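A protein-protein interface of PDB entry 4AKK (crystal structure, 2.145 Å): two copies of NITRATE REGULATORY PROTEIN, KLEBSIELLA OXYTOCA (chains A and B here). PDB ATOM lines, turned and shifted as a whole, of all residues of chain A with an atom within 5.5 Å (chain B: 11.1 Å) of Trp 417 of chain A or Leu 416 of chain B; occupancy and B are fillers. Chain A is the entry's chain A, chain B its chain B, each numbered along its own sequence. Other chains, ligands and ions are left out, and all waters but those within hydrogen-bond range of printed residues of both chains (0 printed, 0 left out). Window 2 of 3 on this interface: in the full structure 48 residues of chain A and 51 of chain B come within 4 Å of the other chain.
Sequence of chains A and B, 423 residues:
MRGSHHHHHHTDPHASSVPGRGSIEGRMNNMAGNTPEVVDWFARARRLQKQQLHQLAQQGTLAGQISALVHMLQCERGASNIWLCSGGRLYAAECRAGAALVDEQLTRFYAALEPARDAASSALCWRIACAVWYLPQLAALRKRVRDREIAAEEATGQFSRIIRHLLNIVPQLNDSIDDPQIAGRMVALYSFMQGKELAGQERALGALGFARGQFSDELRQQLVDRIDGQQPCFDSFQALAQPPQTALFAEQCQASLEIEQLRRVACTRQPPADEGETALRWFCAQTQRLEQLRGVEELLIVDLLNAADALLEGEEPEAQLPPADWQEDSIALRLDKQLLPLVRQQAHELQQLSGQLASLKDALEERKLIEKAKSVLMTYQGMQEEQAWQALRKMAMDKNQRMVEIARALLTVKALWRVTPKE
O of Leu 377 of chain B lies within hydrogen-bond range of N of Met 383 of chain B (3.3 Å).
The side-chain amide oxygen (OE1) of Gln 381 of chain B is in hydrogen-bond range of the indole nitrogen (NE1) of Trp 417 of chain B, at 3.3 Å.
Among the printed residues, pairs that only touch across the chains: Met 395 of chain A with Leu 416 of chain B, Leu 416 of chain A with Trp 417 of chain B, Leu 416 of chain A with Gln 381 of chain B, Trp 417 of chain A with Leu 416 of chain B, Leu 416 of chain A with Leu 377 of chain B, Leu 377 of chain A with Leu 416 of chain B, Leu 416 of chain A with Leu 410 of chain B, Val 413 of chain A with Leu 410 of chain B, Leu 410 of chain A with Val 413 of chain B, Trp 417 of chain A with Trp 417 of chain B, Val 413 of chain A with Ala 409 of chain B, Leu 416 of chain A with Met 395 of chain B and Met 395 of chain A with Val 413 of chain B.
Of chain B, only Leu 416 (3.6 Å) and Trp 417 (3.9 Å) come within 4 Å of Trp 417 of chain A.
Of chain A, only Leu 377, Met 395 and Trp 417 come within 4 Å of Leu 416 of chain B.
No residue of chain B comes within 4 Å of Tyr 380 of chain A.
No residue of chain B comes within 4 Å of Ala 415 of chain A.
Leu 416 of chain A touches just these residues of chain B: Leu 377 (3.8 Å), Gln 381 (3.5 Å), Met 395 (3.9 Å), Leu 410 (3.8 Å) and Trp 417 (3.4 Å).
Of the printed residues of chain B, Leu 377 of chain A touches Leu 416 (3.8 Å).
Of the printed residues of chain A, Leu 410 of chain B touches Val 413 and Leu 416.
Of the printed residues of chain A, Trp 417 of chain B touches Leu 416 and Trp 417.
Gln 381 of chain A touches none of the printed residues of chain B.
The nearest residue of chain A that does not touch Leu 416 of chain B is Gln 381 of chain A (4.1 Å).
Printed residues of chain A that touch a printed residue of chain B: Leu 377, Met 395, Leu 410, Val 413, Leu 416 and Trp 417.
Of the 17 printed residues of chain B, 8 touch a printed residue of chain A.
Hydrophobic or aromatic side chains of chain B within 4 Å of the printed part of chain A: Leu 377, Met 395, Ala 409, Leu 410, Val 413, Leu 416 and Trp 417.
Among the printed residues, no Asp or Glu carboxylate lies within 4 Å of a Lys or Arg side-chain nitrogen of the other chain.
Leu 377 of chain A touches Leu 416 of chain B, and with the chains exchanged Leu 416 of chain A touches Leu 377 of chain B.
Met 395 of chain A touches Val 413 of chain B, but with the chains exchanged Val 413 of chain A does not touch Met 395 of chain B (4.1 Å).
Leu 416 of chain A touches Leu 410 of chain B, but with the chains exchanged Leu 410 of chain A does not touch Leu 416 of chain B (4.1 Å).
Trp 417 of chain A touches its own counterpart, Trp 417 of chain B.
11 positions are printed for both chains.
Of the 13 pairs that touch across the chains among the printed residues, 9 have their exchanged pair printed and touching as well.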
ATOM      1  N   VAL A 376     -28.930  13.060  17.074  1.00  0.00           N
ATOM      2  CA  VAL A 376     -29.477  11.720  16.889  1.00  0.00           C
ATOM      3  C   VAL A 376     -29.208  10.856  18.112  1.00  0.00           C
ATOM      4  O   VAL A 376     -30.096  10.149  18.585  1.00  0.00           O
ATOM      5  CB  VAL A 376     -28.915  11.025  15.630  1.00  0.00           C
ATOM      6  CG1 VAL A 376     -29.206   9.523  15.676  1.00  0.00           C
ATOM      7  CG2 VAL A 376     -29.500  11.659  14.366  1.00  0.00           C
ATOM      8  N   LEU A 377     -27.979  10.911  18.615  1.00  0.00           N
ATOM      9  CA  LEU A 377     -27.612  10.169  19.815  1.00  0.00           C
ATOM     10  C   LEU A 377     -28.323  10.722  21.052  1.00  0.00           C
ATOM     11  O   LEU A 377     -28.696   9.973  21.952  1.00  0.00           O
ATOM     12  CB  LEU A 377     -26.094  10.192  20.017  1.00  0.00           C
ATOM     13  CG  LEU A 377     -25.260   9.552  18.899  1.00  0.00           C
ATOM     14  CD1 LEU A 377     -23.779   9.758  19.113  1.00  0.00           C
ATOM     15  CD2 LEU A 377     -25.585   8.076  18.780  1.00  0.00           C
ATOM     16  N   TYR A 380     -32.416   9.474  20.341  1.00  0.00           N
ATOM     17  CA  TYR A 380     -32.782   8.073  20.221  1.00  0.00           C
ATOM     18  C   TYR A 380     -31.975   7.185  21.144  1.00  0.00           C
ATOM     19  O   TYR A 380     -32.137   5.968  21.135  1.00  0.00           O
ATOM     20  CB  TYR A 380     -32.641   7.615  18.770  1.00  0.00           C
ATOM     21  CG  TYR A 380     -33.515   8.418  17.841  1.00  0.00           C
ATOM     22  CD1 TYR A 380     -34.838   8.058  17.616  1.00  0.00           C
ATOM     23  CD2 TYR A 380     -33.032   9.560  17.219  1.00  0.00           C
ATOM     24  CE1 TYR A 380     -35.649   8.805  16.781  1.00  0.00           C
ATOM     25  CE2 TYR A 380     -33.835  10.312  16.380  1.00  0.00           C
ATOM     26  CZ  TYR A 380     -35.142   9.928  16.165  1.00  0.00           C
ATOM     27  OH  TYR A 380     -35.942  10.676  15.329  1.00  0.00           O
ATOM     28  N   GLN A 381     -31.115   7.788  21.955  1.00  0.00           N
ATOM     29  CA  GLN A 381     -30.247   6.994  22.814  1.00  0.00           C
ATOM     30  C   GLN A 381     -30.013   7.642  24.177  1.00  0.00           C
ATOM     31  O   GLN A 381     -29.322   7.085  25.028  1.00  0.00           O
ATOM     32  CB  GLN A 381     -28.928   6.709  22.100  1.00  0.00           C
ATOM     33  CG  GLN A 381     -28.280   5.405  22.508  1.00  0.00           C
ATOM     34  CD  GLN A 381     -27.592   4.732  21.345  1.00  0.00           C
ATOM     35  OE1 GLN A 381     -27.778   5.125  20.193  1.00  0.00           O
ATOM     36  NE2 GLN A 381     -26.798   3.707  21.636  1.00  0.00           N
ATOM     37  N   MET A 395     -15.928   6.239  18.181  1.00  0.00           N
ATOM     38  CA  MET A 395     -16.164   5.421  16.986  1.00  0.00           C
ATOM     39  C   MET A 395     -15.152   5.743  15.884  1.00  0.00           C
ATOM     40  O   MET A 395     -14.764   4.868  15.124  1.00  0.00           O
ATOM     41  CB  MET A 395     -17.600   5.579  16.467  1.00  0.00           C
ATOM     42  CG  MET A 395     -18.588   4.528  16.985  1.00  0.00           C
ATOM     43  SD  MET A 395     -20.311   4.830  16.486  1.00  0.00           S
ATOM     44  CE  MET A 395     -20.690   6.169  17.598  1.00  0.00           C
ATOM     45  N   LEU A 410     -23.824   7.721  10.345  1.00  0.00           N
ATOM     46  CA  LEU A 410     -25.001   7.600  11.211  1.00  0.00           C
ATOM     47  C   LEU A 410     -26.257   8.250  10.621  1.00  0.00           C
ATOM     48  O   LEU A 410     -27.360   7.728  10.777  1.00  0.00           O
ATOM     49  CB  LEU A 410     -24.718   8.154  12.612  1.00  0.00           C
ATOM     50  CG  LEU A 410     -25.888   8.281  13.598  1.00  0.00           C
ATOM     51  CD1 LEU A 410     -26.568   6.939  13.824  1.00  0.00           C
ATOM     52  CD2 LEU A 410     -25.424   8.876  14.930  1.00  0.00           C
ATOM     53  N   VAL A 413     -27.981   6.052   7.942  1.00  0.00           N
ATOM     54  CA  VAL A 413     -28.799   4.919   8.354  1.00  0.00           C
ATOM     55  C   VAL A 413     -29.788   5.233   9.484  1.00  0.00           C
ATOM     56  O   VAL A 413     -30.353   4.322  10.091  1.00  0.00           O
ATOM     57  CB  VAL A 413     -27.919   3.741   8.823  1.00  0.00           C
ATOM     58  CG1 VAL A 413     -26.951   3.314   7.733  1.00  0.00           C
ATOM     59  CG2 VAL A 413     -27.181   4.112  10.089  1.00  0.00           C
ATOM     60  N   LYS A 414     -30.010   6.505   9.783  1.00  0.00           N
ATOM     61  CA  LYS A 414     -30.764   6.812  11.006  1.00  0.00           C
ATOM     62  C   LYS A 414     -32.236   6.399  10.908  1.00  0.00           C
ATOM     63  O   LYS A 414     -32.939   6.358  11.915  1.00  0.00           O
ATOM     64  CB  LYS A 414     -30.595   8.271  11.467  1.00  0.00           C
ATOM     65  CG  LYS A 414     -31.073   9.302  10.474  1.00  0.00           C
ATOM     66  CD  LYS A 414     -31.261  10.663  11.135  1.00  0.00           C
ATOM     67  CE  LYS A 414     -31.435  11.738  10.080  1.00  0.00           C
ATOM     68  NZ  LYS A 414     -32.587  11.453   9.171  1.00  0.00           N
ATOM     69  N   ALA A 415     -32.686   6.070   9.702  1.00  0.00           N
ATOM     70  CA  ALA A 415     -34.002   5.471   9.531  1.00  0.00           C
ATOM     71  C   ALA A 415     -34.114   4.171  10.327  1.00  0.00           C
ATOM     72  O   ALA A 415     -35.211   3.709  10.617  1.00  0.00           O
ATOM     73  CB  ALA A 415     -34.285   5.215   8.066  1.00  0.00           C
ATOM     74  N   LEU A 416     -32.974   3.586  10.676  1.00  0.00           N
ATOM     75  CA  LEU A 416     -32.946   2.371  11.483  1.00  0.00           C
ATOM     76  C   LEU A 416     -33.217   2.644  12.961  1.00  0.00           C
ATOM     77  O   LEU A 416     -33.773   1.799  13.662  1.00  0.00           O
ATOM     78  CB  LEU A 416     -31.603   1.667  11.332  1.00  0.00           C
ATOM     79  CG  LEU A 416     -31.396   0.933  10.013  1.00  0.00           C
ATOM     80  CD1 LEU A 416     -29.969   0.442   9.918  1.00  0.00           C
ATOM     81  CD2 LEU A 416     -32.363  -0.221   9.921  1.00  0.00           C
ATOM     82  N   TRP A 417     -32.812   3.814  13.440  1.00  0.00           N
ATOM     83  CA  TRP A 417     -33.131   4.217  14.806  1.00  0.00           C
ATOM     84  C   TRP A 417     -34.573   4.717  14.922  1.00  0.00           C
ATOM     85  O   TRP A 417     -35.225   4.543  15.954  1.00  0.00           O
ATOM     86  CB  TRP A 417     -32.164   5.295  15.294  1.00  0.00           C
ATOM     87  CG  TRP A 417     -31.070   4.763  16.164  1.00  0.00           C
ATOM     88  CD1 TRP A 417     -29.724   4.915  15.980  1.00  0.00           C
ATOM     89  CD2 TRP A 417     -31.227   3.987  17.360  1.00  0.00           C
ATOM     90  NE1 TRP A 417     -29.035   4.286  16.991  1.00  0.00           N
ATOM     91  CE2 TRP A 417     -29.932   3.708  17.851  1.00  0.00           C
ATOM     92  CE3 TRP A 417     -32.336   3.503  18.067  1.00  0.00           C
ATOM     93  CZ2 TRP A 417     -29.717   2.963  19.015  1.00  0.00           C
ATOM     94  CZ3 TRP A 417     -32.120   2.764  19.223  1.00  0.00           C
ATOM     95  CH2 TRP A 417     -30.821   2.502  19.684  1.00  0.00           C
ATOM     96  N   ARG A 418     -35.060   5.333  13.846  1.00  0.00           N
ATOM     97  CA  ARG A 418     -36.395   5.924  13.807  1.00  0.00           C
ATOM     98  C   ARG A 418     -37.479   4.895  14.105  1.00  0.00           C
ATOM     99  O   ARG A 418     -38.488   4.820  13.400  1.00  0.00           O
ATOM    100  CB  ARG A 418     -36.645   6.560  12.437  1.00  0.00           C
ATOM    101  CG  ARG A 418     -37.814   7.525  12.392  1.00  0.00           C
ATOM    102  CD  ARG A 418     -38.247   7.777  10.957  1.00  0.00           C
ATOM    103  NE  ARG A 418     -37.101   7.952  10.068  1.00  0.00           N
ATOM    104  CZ  ARG A 418     -36.494   9.114   9.848  1.00  0.00           C
ATOM    105  NH1 ARG A 418     -36.923  10.213  10.456  1.00  0.00           N
ATOM    106  NH2 ARG A 418     -35.457   9.180   9.022  1.00  0.00           N
ATOM    107  N   VAL B 376     -26.329  -7.983  10.235  1.00  0.00           N
ATOM    108  CA  VAL B 376     -26.589  -7.033  11.306  1.00  0.00           C
ATOM    109  C   VAL B 376     -28.079  -6.773  11.465  1.00  0.00           C
ATOM    110  O   VAL B 376     -28.579  -6.700  12.583  1.00  0.00           O
ATOM    111  CB  VAL B 376     -25.878  -5.702  11.047  1.00  0.00           C
ATOM    112  CG1 VAL B 376     -26.303  -4.656  12.078  1.00  0.00           C
ATOM    113  CG2 VAL B 376     -24.375  -5.914  11.052  1.00  0.00           C
ATOM    114  N   LEU B 377     -28.783  -6.626  10.344  1.00  0.00           N
ATOM    115  CA  LEU B 377     -30.215  -6.376  10.384  1.00  0.00           C
ATOM    116  C   LEU B 377     -30.955  -7.645  10.774  1.00  0.00           C
ATOM    117  O   LEU B 377     -31.973  -7.595  11.454  1.00  0.00           O
ATOM    118  CB  LEU B 377     -30.723  -5.867   9.031  1.00  0.00           C
ATOM    119  CG  LEU B 377     -30.207  -4.502   8.569  1.00  0.00           C
ATOM    120  CD1 LEU B 377     -30.840  -4.111   7.247  1.00  0.00           C
ATOM    121  CD2 LEU B 377     -30.480  -3.451   9.620  1.00  0.00           C
ATOM    122  N   TYR B 380     -29.863  -8.003  14.925  1.00  0.00           N
ATOM    123  CA  TYR B 380     -30.277  -6.984  15.884  1.00  0.00           C
ATOM    124  C   TYR B 380     -31.676  -6.453  15.653  1.00  0.00           C
ATOM    125  O   TYR B 380     -32.194  -5.697  16.470  1.00  0.00           O
ATOM    126  CB  TYR B 380     -29.292  -5.824  15.864  1.00  0.00           C
ATOM    127  CG  TYR B 380     -27.916  -6.224  16.320  1.00  0.00           C
ATOM    128  CD1 TYR B 380     -27.617  -6.330  17.672  1.00  0.00           C
ATOM    129  CD2 TYR B 380     -26.922  -6.518  15.401  1.00  0.00           C
ATOM    130  CE1 TYR B 380     -26.359  -6.707  18.094  1.00  0.00           C
ATOM    131  CE2 TYR B 380     -25.663  -6.893  15.812  1.00  0.00           C
ATOM    132  CZ  TYR B 380     -25.385  -6.987  17.160  1.00  0.00           C
ATOM    133  OH  TYR B 380     -24.126  -7.361  17.569  1.00  0.00           O
ATOM    134  N   GLN B 381     -32.289  -6.842  14.544  1.00  0.00           N
ATOM    135  CA  GLN B 381     -33.580  -6.278  14.181  1.00  0.00           C
ATOM    136  C   GLN B 381     -34.578  -7.361  13.793  1.00  0.00           C
ATOM    137  O   GLN B 381     -35.737  -7.071  13.502  1.00  0.00           O
ATOM    138  CB  GLN B 381     -33.404  -5.279  13.048  1.00  0.00           C
ATOM    139  CG  GLN B 381     -34.249  -4.042  13.182  1.00  0.00           C
ATOM    140  CD  GLN B 381     -33.431  -2.790  12.966  1.00  0.00           C
ATOM    141  OE1 GLN B 381     -32.211  -2.798  13.152  1.00  0.00           O
ATOM    142  NE2 GLN B 381     -34.093  -1.703  12.574  1.00  0.00           N
ATOM    143  N   MET B 383     -34.850  -9.230  11.162  1.00  0.00           N
ATOM    144  CA  MET B 383     -35.321  -9.223   9.784  1.00  0.00           C
ATOM    145  C   MET B 383     -34.996 -10.554   9.126  1.00  0.00           C
ATOM    146  O   MET B 383     -34.050 -11.237   9.515  1.00  0.00           O
ATOM    147  CB  MET B 383     -34.673  -8.085   8.988  1.00  0.00           C
ATOM    148  CG  MET B 383     -35.182  -6.693   9.320  1.00  0.00           C
ATOM    149  SD  MET B 383     -34.612  -5.466   8.119  1.00  0.00           S
ATOM    150  CE  MET B 383     -35.241  -3.967   8.836  1.00  0.00           C
ATOM    151  N   ALA B 391     -34.451  -3.724   2.858  1.00  0.00           N
ATOM    152  CA  ALA B 391     -34.288  -2.569   3.738  1.00  0.00           C
ATOM    153  C   ALA B 391     -33.080  -1.739   3.299  1.00  0.00           C
ATOM    154  O   ALA B 391     -33.167  -0.523   3.180  1.00  0.00           O
ATOM    155  CB  ALA B 391     -34.147  -3.013   5.192  1.00  0.00           C
ATOM    156  N   MET B 395     -33.123   2.077   1.775  1.00  0.00           N
ATOM    157  CA  MET B 395     -32.276   3.162   2.283  1.00  0.00           C
ATOM    158  C   MET B 395     -31.381   3.758   1.184  1.00  0.00           C
ATOM    159  O   MET B 395     -31.147   4.961   1.147  1.00  0.00           O
ATOM    160  CB  MET B 395     -31.438   2.689   3.475  1.00  0.00           C
ATOM    161  CG  MET B 395     -32.105   2.903   4.837  1.00  0.00           C
ATOM    162  SD  MET B 395     -31.125   2.321   6.252  1.00  0.00           S
ATOM    163  CE  MET B 395     -31.381   0.570   6.084  1.00  0.00           C
ATOM    164  N   LYS B 399     -31.685   7.748   0.266  1.00  0.00           N
ATOM    165  CA  LYS B 399     -30.511   8.584   0.517  1.00  0.00           C
ATOM    166  C   LYS B 399     -29.728   8.852  -0.760  1.00  0.00           C
ATOM    167  O   LYS B 399     -28.719   9.553  -0.728  1.00  0.00           O
ATOM    168  CB  LYS B 399     -29.577   7.920   1.545  1.00  0.00           C
ATOM    169  CG  LYS B 399     -30.212   7.746   2.908  1.00  0.00           C
ATOM    170  CD  LYS B 399     -30.565   9.107   3.507  1.00  0.00           C
ATOM    171  CE  LYS B 399     -31.223   8.962   4.867  1.00  0.00           C
ATOM    172  NZ  LYS B 399     -31.591  10.276   5.463  1.00  0.00           N
ATOM    173  N   ALA B 409     -21.850   2.210   5.733  1.00  0.00           N
ATOM    174  CA  ALA B 409     -22.328   3.130   6.767  1.00  0.00           C
ATOM    175  C   ALA B 409     -22.832   2.372   7.999  1.00  0.00           C
ATOM    176  O   ALA B 409     -22.465   2.689   9.132  1.00  0.00           O
ATOM    177  CB  ALA B 409     -23.420   4.024   6.212  1.00  0.00           C
ATOM    178  N   LEU B 410     -23.667   1.365   7.767  1.00  0.00           N
ATOM    179  CA  LEU B 410     -24.194   0.541   8.856  1.00  0.00           C
ATOM    180  C   LEU B 410     -23.075  -0.147   9.637  1.00  0.00           C
ATOM    181  O   LEU B 410     -23.133  -0.258  10.862  1.00  0.00           O
ATOM    182  CB  LEU B 410     -25.153  -0.520   8.307  1.00  0.00           C
ATOM    183  CG  LEU B 410     -25.861  -1.437   9.313  1.00  0.00           C
ATOM    184  CD1 LEU B 410     -26.396  -0.652  10.499  1.00  0.00           C
ATOM    185  CD2 LEU B 410     -26.988  -2.224   8.636  1.00  0.00           C
ATOM    186  N   LEU B 411     -22.063  -0.626   8.921  1.00  0.00           N
ATOM    187  CA  LEU B 411     -20.968  -1.327   9.568  1.00  0.00           C
ATOM    188  C   LEU B 411     -20.051  -0.382  10.345  1.00  0.00           C
ATOM    189  O   LEU B 411     -19.384  -0.816  11.283  1.00  0.00           O
ATOM    190  CB  LEU B 411     -20.153  -2.142   8.555  1.00  0.00           C
ATOM    191  CG  LEU B 411     -20.891  -3.241   7.779  1.00  0.00           C
ATOM    192  CD1 LEU B 411     -19.966  -3.865   6.737  1.00  0.00           C
ATOM    193  CD2 LEU B 411     -21.475  -4.298   8.716  1.00  0.00           C
ATOM    194  N   THR B 412     -19.999   0.895   9.973  1.00  0.00           N
ATOM    195  CA  THR B 412     -19.112   1.779  10.717  1.00  0.00           C
ATOM    196  C   THR B 412     -19.698   2.197  12.064  1.00  0.00           C
ATOM    197  O   THR B 412     -18.955   2.466  13.003  1.00  0.00           O
ATOM    198  CB  THR B 412     -18.584   3.020   9.929  1.00  0.00           C
ATOM    199  OG1 THR B 412     -19.326   4.185  10.281  1.00  0.00           O
ATOM    200  CG2 THR B 412     -18.603   2.813   8.445  1.00  0.00           C
ATOM    201  N   VAL B 413     -21.021   2.236  12.168  1.00  0.00           N
ATOM    202  CA  VAL B 413     -21.643   2.668  13.414  1.00  0.00           C
ATOM    203  C   VAL B 413     -22.282   1.501  14.148  1.00  0.00           C
ATOM    204  O   VAL B 413     -23.207   1.676  14.932  1.00  0.00           O
ATOM    205  CB  VAL B 413     -22.709   3.749  13.171  1.00  0.00           C
ATOM    206  CG1 VAL B 413     -22.093   4.945  12.477  1.00  0.00           C
ATOM    207  CG2 VAL B 413     -23.845   3.180  12.351  1.00  0.00           C
ATOM    208  N   LYS B 414     -21.784   0.301  13.901  1.00  0.00           N
ATOM    209  CA  LYS B 414     -22.423  -0.869  14.475  1.00  0.00           C
ATOM    210  C   LYS B 414     -22.219  -0.960  15.986  1.00  0.00           C
ATOM    211  O   LYS B 414     -22.894  -1.734  16.661  1.00  0.00           O
ATOM    212  CB  LYS B 414     -21.964  -2.146  13.773  1.00  0.00           C
ATOM    213  CG  LYS B 414     -22.988  -3.267  13.833  1.00  0.00           C
ATOM    214  CD  LYS B 414     -22.460  -4.484  13.111  1.00  0.00           C
ATOM    215  CE  LYS B 414     -20.954  -4.609  13.264  1.00  0.00           C
ATOM    216  NZ  LYS B 414     -20.371  -5.504  12.232  1.00  0.00           N
ATOM    217  N   ALA B 415     -21.304  -0.164  16.526  1.00  0.00           N
ATOM    218  CA  ALA B 415     -21.167  -0.094  17.974  1.00  0.00           C
ATOM    219  C   ALA B 415     -22.480   0.359  18.622  1.00  0.00           C
ATOM    220  O   ALA B 415     -22.743   0.059  19.783  1.00  0.00           O
ATOM    221  CB  ALA B 415     -20.021   0.828  18.370  1.00  0.00           C
ATOM    222  N   LEU B 416     -23.311   1.065  17.864  1.00  0.00           N
ATOM    223  CA  LEU B 416     -24.591   1.553  18.375  1.00  0.00           C
ATOM    224  C   LEU B 416     -25.714   0.507  18.355  1.00  0.00           C
ATOM    225  O   LEU B 416     -26.831   0.784  18.793  1.00  0.00           O
ATOM    226  CB  LEU B 416     -25.031   2.784  17.585  1.00  0.00           C
ATOM    227  CG  LEU B 416     -24.476   4.143  18.011  1.00  0.00           C
ATOM    228  CD1 LEU B 416     -23.098   3.990  18.614  1.00  0.00           C
ATOM    229  CD2 LEU B 416     -24.433   5.080  16.811  1.00  0.00           C
ATOM    230  N   TRP B 417     -25.425  -0.686  17.844  1.00  0.00           N
ATOM    231  CA  TRP B 417     -26.441  -1.738  17.741  1.00  0.00           C
ATOM    232  C   TRP B 417     -26.359  -2.775  18.861  1.00  0.00           C
ATOM    233  O   TRP B 417     -25.441  -2.752  19.683  1.00  0.00           O
ATOM    234  CB  TRP B 417     -26.370  -2.428  16.374  1.00  0.00           C
ATOM    235  CG  TRP B 417     -27.395  -1.924  15.394  1.00  0.00           C
ATOM    236  CD1 TRP B 417     -28.373  -2.657  14.780  1.00  0.00           C
ATOM    237  CD2 TRP B 417     -27.554  -0.576  14.929  1.00  0.00           C
ATOM    238  NE1 TRP B 417     -29.124  -1.851  13.955  1.00  0.00           N
ATOM    239  CE2 TRP B 417     -28.642  -0.570  14.031  1.00  0.00           C
ATOM    240  CE3 TRP B 417     -26.881   0.625  15.181  1.00  0.00           C
ATOM    241  CZ2 TRP B 417     -29.071   0.593  13.386  1.00  0.00           C
ATOM    242  CZ3 TRP B 417     -27.310   1.779  14.539  1.00  0.00           C
ATOM    243  CH2 TRP B 417     -28.393   1.753  13.653  1.00  0.00           C
